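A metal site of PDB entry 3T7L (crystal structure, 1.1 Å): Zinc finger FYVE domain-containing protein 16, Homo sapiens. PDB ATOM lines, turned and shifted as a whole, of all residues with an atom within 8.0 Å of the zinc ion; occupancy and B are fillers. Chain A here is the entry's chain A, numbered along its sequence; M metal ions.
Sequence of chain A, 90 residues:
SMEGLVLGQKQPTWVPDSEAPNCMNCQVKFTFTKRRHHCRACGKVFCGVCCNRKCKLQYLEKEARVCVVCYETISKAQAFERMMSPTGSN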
ATOM      1  N   ASN A  22      14.226 -28.692 -12.342  1.00  0.00           N
ATOM      2  CA  ASN A  22      13.822 -27.294 -12.547  1.00  0.00           C
ATOM      3  C   ASN A  22      14.615 -26.633 -13.648  1.00  0.00           C
ATOM      4  O   ASN A  22      15.788 -26.965 -13.913  1.00  0.00           O
ATOM      5  CB  ASN A  22      14.048 -26.485 -11.245  1.00  0.00           C
ATOM      6  CG  ASN A  22      13.204 -26.926 -10.101  1.00  0.00           C
ATOM      7  OD1 ASN A  22      13.484 -27.963  -9.497  1.00  0.00           O
ATOM      8  ND2 ASN A  22      12.179 -26.157  -9.758  1.00  0.00           N
ATOM      9  N   CYS A  23      14.003 -25.675 -14.327  1.00  0.00           N
ATOM     10  CA  CYS A  23      14.701 -24.884 -15.326  1.00  0.00           C
ATOM     11  C   CYS A  23      15.908 -24.249 -14.726  1.00  0.00           C
ATOM     12  O   CYS A  23      15.837 -23.589 -13.689  1.00  0.00           O
ATOM     13  CB  CYS A  23      13.743 -23.853 -15.891  1.00  0.00           C
ATOM     14  SG  CYS A  23      14.575 -22.745 -17.097  1.00  0.00           S
ATOM     15  N   MET A  24      17.049 -24.391 -15.409  1.00  0.00           N
ATOM     16  CA  MET A  24      18.315 -23.912 -14.887  1.00  0.00           C
ATOM     17  C   MET A  24      18.543 -22.446 -15.156  1.00  0.00           C
ATOM     18  O   MET A  24      19.615 -21.925 -14.809  1.00  0.00           O
ATOM     19  CB  MET A  24      19.443 -24.807 -15.408  1.00  0.00           C
ATOM     20  CG  MET A  24      19.314 -26.217 -14.866  1.00  0.00           C
ATOM     21  SD  MET A  24      20.552 -27.340 -15.466  1.00  0.00           S
ATOM     22  CE  MET A  24      19.845 -28.858 -14.834  1.00  0.00           C
ATOM     23  N   ASN A  25      17.578 -21.750 -15.746  1.00  0.00           N
ATOM     24  CA  ASN A  25      17.550 -20.292 -15.760  1.00  0.00           C
ATOM     25  C   ASN A  25      16.516 -19.744 -14.784  1.00  0.00           C
ATOM     26  O   ASN A  25      16.888 -19.037 -13.833  1.00  0.00           O
ATOM     27  CB  ASN A  25      17.310 -19.732 -17.141  1.00  0.00           C
ATOM     28  CG  ASN A  25      17.363 -18.221 -17.154  1.00  0.00           C
ATOM     29  OD1 ASN A  25      18.385 -17.646 -16.769  1.00  0.00           O
ATOM     30  ND2 ASN A  25      16.290 -17.565 -17.549  1.00  0.00           N
ATOM     31  N   CYS A  26      15.246 -20.022 -14.985  1.00  0.00           N
ATOM     32  CA  CYS A  26      14.167 -19.330 -14.246  1.00  0.00           C
ATOM     33  C   CYS A  26      13.675 -20.078 -13.036  1.00  0.00           C
ATOM     34  O   CYS A  26      12.869 -19.508 -12.281  1.00  0.00           O
ATOM     35  CB  CYS A  26      12.988 -19.008 -15.150  1.00  0.00           C
ATOM     36  SG  CYS A  26      11.961 -20.490 -15.579  1.00  0.00           S
ATOM     37  N   GLN A  27      14.120 -21.297 -12.820  1.00  0.00           N
ATOM     38  CA  GLN A  27      13.790 -22.122 -11.645  1.00  0.00           C
ATOM     39  C   GLN A  27      12.401 -22.763 -11.659  1.00  0.00           C
ATOM     40  O   GLN A  27      12.070 -23.479 -10.728  1.00  0.00           O
ATOM     41  CB  GLN A  27      14.025 -21.402 -10.295  1.00  0.00           C
ATOM     42  CG  GLN A  27      15.419 -20.802 -10.174  1.00  0.00           C
ATOM     43  CD  GLN A  27      15.778 -20.267  -8.831  1.00  0.00           C
ATOM     44  OE1 GLN A  27      14.983 -19.979  -8.001  1.00  0.00           O
ATOM     45  NE2 GLN A  27      17.079 -19.997  -8.674  1.00  0.00           N
ATOM     46  N   VAL A  28      11.628 -22.590 -12.714  1.00  0.00           N
ATOM     47  CA  VAL A  28      10.320 -23.235 -12.768  1.00  0.00           C
ATOM     48  C   VAL A  28      10.470 -24.761 -12.702  1.00  0.00           C
ATOM     49  O   VAL A  28      11.382 -25.328 -13.302  1.00  0.00           O
ATOM     50  CB  VAL A  28       9.508 -22.780 -13.998  1.00  0.00           C
ATOM     51  CG1 VAL A  28      10.025 -23.383 -15.346  1.00  0.00           C
ATOM     52  CG2 VAL A  28       7.997 -23.072 -13.838  1.00  0.00           C
ATOM     53  N   LYS A  29       9.546 -25.434 -12.043  1.00  0.00           N
ATOM     54  CA  LYS A  29       9.566 -26.874 -11.952  1.00  0.00           C
ATOM     55  C   LYS A  29       9.036 -27.507 -13.227  1.00  0.00           C
ATOM     56  O   LYS A  29       8.007 -27.111 -13.768  1.00  0.00           O
ATOM     57  CB  LYS A  29       8.706 -27.307 -10.739  1.00  0.00           C
ATOM     58  CG  LYS A  29       8.778 -28.802 -10.480  1.00  0.00           C
ATOM     59  CD  LYS A  29       8.035 -29.235  -9.284  1.00  0.00           C
ATOM     60  CE  LYS A  29       8.186 -30.717  -9.011  1.00  0.00           C
ATOM     61  NZ  LYS A  29       9.584 -31.181  -8.933  1.00  0.00           N
ATOM     62  N   PHE A  30       9.762 -28.502 -13.748  1.00  0.00           N
ATOM     63  CA  PHE A  30       9.259 -29.279 -14.882  1.00  0.00           C
ATOM     64  C   PHE A  30       8.088 -30.119 -14.439  1.00  0.00           C
ATOM     65  O   PHE A  30       8.083 -30.699 -13.323  1.00  0.00           O
ATOM     66  CB  PHE A  30      10.350 -30.128 -15.504  1.00  0.00           C
ATOM     67  CG  PHE A  30      11.476 -29.296 -16.101  1.00  0.00           C
ATOM     68  CD1 PHE A  30      11.234 -28.478 -17.165  1.00  0.00           C
ATOM     69  CD2 PHE A  30      12.742 -29.349 -15.589  1.00  0.00           C
ATOM     70  CE1 PHE A  30      12.292 -27.709 -17.696  1.00  0.00           C
ATOM     71  CE2 PHE A  30      13.780 -28.602 -16.124  1.00  0.00           C
ATOM     72  CZ  PHE A  30      13.534 -27.802 -17.176  1.00  0.00           C
ATOM     73  N   LYS A  34       5.130 -28.847 -18.696  1.00  0.00           N
ATOM     74  CA  LYS A  34       6.256 -27.932 -18.778  1.00  0.00           C
ATOM     75  C   LYS A  34       7.489 -28.788 -18.919  1.00  0.00           C
ATOM     76  O   LYS A  34       8.076 -29.250 -17.955  1.00  0.00           O
ATOM     77  CB  LYS A  34       6.323 -27.055 -17.582  1.00  0.00           C
ATOM     78  CG  LYS A  34       7.234 -25.892 -17.830  1.00  0.00           C
ATOM     79  CD  LYS A  34       7.167 -24.964 -16.677  1.00  0.00           C
ATOM     80  CE  LYS A  34       5.763 -24.492 -16.430  1.00  0.00           C
ATOM     81  NZ  LYS A  34       5.320 -23.530 -17.469  1.00  0.00           N
ATOM     82  N   VAL A  45      19.571 -27.571 -18.785  1.00  0.00           N
ATOM     83  CA  VAL A  45      18.183 -27.951 -19.056  1.00  0.00           C
ATOM     84  C   VAL A  45      17.255 -26.820 -18.675  1.00  0.00           C
ATOM     85  O   VAL A  45      17.368 -26.252 -17.593  1.00  0.00           O
ATOM     86  CB  VAL A  45      17.783 -29.204 -18.280  1.00  0.00           C
ATOM     87  CG1 VAL A  45      16.463 -29.750 -18.792  1.00  0.00           C
ATOM     88  CG2 VAL A  45      18.888 -30.301 -18.370  1.00  0.00           C
ATOM     89  N   PHE A  46      16.371 -26.473 -19.609  1.00  0.00           N
ATOM     90  CA  PHE A  46      15.548 -25.270 -19.534  1.00  0.00           C
ATOM     91  C   PHE A  46      14.117 -25.521 -19.921  1.00  0.00           C
ATOM     92  O   PHE A  46      13.826 -26.456 -20.659  1.00  0.00           O
ATOM     93  CB  PHE A  46      16.137 -24.229 -20.499  1.00  0.00           C
ATOM     94  CG  PHE A  46      17.547 -23.861 -20.196  1.00  0.00           C
ATOM     95  CD1 PHE A  46      18.601 -24.550 -20.789  1.00  0.00           C
ATOM     96  CD2 PHE A  46      17.841 -22.900 -19.259  1.00  0.00           C
ATOM     97  CE1 PHE A  46      19.916 -24.231 -20.477  1.00  0.00           C
ATOM     98  CE2 PHE A  46      19.156 -22.573 -18.942  1.00  0.00           C
ATOM     99  CZ  PHE A  46      20.204 -23.274 -19.555  1.00  0.00           C
ATOM    100  N   CYS A  47      13.253 -24.641 -19.470  1.00  0.00           N
ATOM    101  CA  CYS A  47      11.898 -24.560 -20.035  1.00  0.00           C
ATOM    102  C   CYS A  47      11.925 -23.917 -21.412  1.00  0.00           C
ATOM    103  O   CYS A  47      12.941 -23.326 -21.815  1.00  0.00           O
ATOM    104  CB  CYS A  47      10.963 -23.811 -19.082  1.00  0.00           C
ATOM    105  SG  CYS A  47      11.208 -22.001 -19.112  1.00  0.00           S
ATOM    106  N   GLY A  48      10.858 -24.043 -22.153  1.00  0.00           N
ATOM    107  CA  GLY A  48      10.854 -23.511 -23.491  1.00  0.00           C
ATOM    108  C   GLY A  48      11.061 -22.010 -23.540  1.00  0.00           C
ATOM    109  O   GLY A  48      11.726 -21.501 -24.451  1.00  0.00           O
ATOM    110  N   VAL A  49      10.461 -21.267 -22.612  1.00  0.00           N
ATOM    111  CA  VAL A  49      10.585 -19.805 -22.575  1.00  0.00           C
ATOM    112  C   VAL A  49      12.024 -19.344 -22.389  1.00  0.00           C
ATOM    113  O   VAL A  49      12.358 -18.240 -22.808  1.00  0.00           O
ATOM    114  CB  VAL A  49       9.687 -19.199 -21.479  1.00  0.00           C
ATOM    115  CG1 VAL A  49      10.095 -17.758 -21.130  1.00  0.00           C
ATOM    116  CG2 VAL A  49       8.221 -19.231 -21.888  1.00  0.00           C
ATOM    117  N   CYS A  50      12.833 -20.155 -21.712  1.00  0.00           N
ATOM    118  CA  CYS A  50      14.254 -19.877 -21.498  1.00  0.00           C
ATOM    119  C   CYS A  50      15.147 -20.492 -22.530  1.00  0.00           C
ATOM    120  O   CYS A  50      16.358 -20.221 -22.510  1.00  0.00           O
ATOM    121  CB  CYS A  50      14.665 -20.326 -20.098  1.00  0.00           C
ATOM    122  SG  CYS A  50      13.802 -19.436 -18.754  1.00  0.00           S
ATOM    123  N   CYS A  51      14.622 -21.278 -23.445  1.00  0.00           N
ATOM    124  CA  CYS A  51      15.450 -21.982 -24.424  1.00  0.00           C
ATOM    125  C   CYS A  51      14.642 -22.291 -25.645  1.00  0.00           C
ATOM    126  O   CYS A  51      14.111 -23.384 -25.775  1.00  0.00           O
ATOM    127  CB  CYS A  51      16.018 -23.239 -23.783  1.00  0.00           C
ATOM    128  SG  CYS A  51      17.161 -24.226 -24.752  1.00  0.00           S
ATOM    129  N   VAL A  68      18.764 -18.712 -23.239  1.00  0.00           N
ATOM    130  CA  VAL A  68      18.786 -17.263 -23.291  1.00  0.00           C
ATOM    131  C   VAL A  68      20.202 -16.690 -23.133  1.00  0.00           C
ATOM    132  O   VAL A  68      20.584 -15.715 -23.757  1.00  0.00           O
ATOM    133  CB  VAL A  68      17.815 -16.679 -22.236  1.00  0.00           C
ATOM    134  CG1 VAL A  68      18.162 -17.195 -20.828  1.00  0.00           C
ATOM    135  CG2 VAL A  68      17.765 -15.140 -22.328  1.00  0.00           C
HETATM  136 ZN    ZN M   1      12.835 -21.214 -17.605  1.00  0.00          ZN
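The backbone NH of Val 28 lies close to the side-chain sulfur of Cys 26 (3.6 Å). The side-chain sulfur of Cys 50 lies close to the side-chain amide nitrogen of Asn 25. O of Cys 50 sits at hydrogen-bond distance from N of Val 68 (2.9 Å). The side-chain sulfur (SG) of Cys 47 sits close to the backbone NH (N) of Val 49 (3.7 Å). The backbone carbonyl oxygen (O) of Val 28 sits at hydrogen-bond distance from the backbone NH (N) of Cys 23. N of Asn 25 lies close to SG of Cys 23, at 3.4 Å.
The nearest printed residue that does not touch the zinc ion is Val 28 (4.2 Å).
The zinc ion is bound by SG of Cys 26 (2.3 Å), SG of Cys 50 (2.3 Å), SG of Cys 47 (2.4 Å) and SG of Cys 23 (2.4 Å). The zinc ion has four donor atoms within binding distance.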
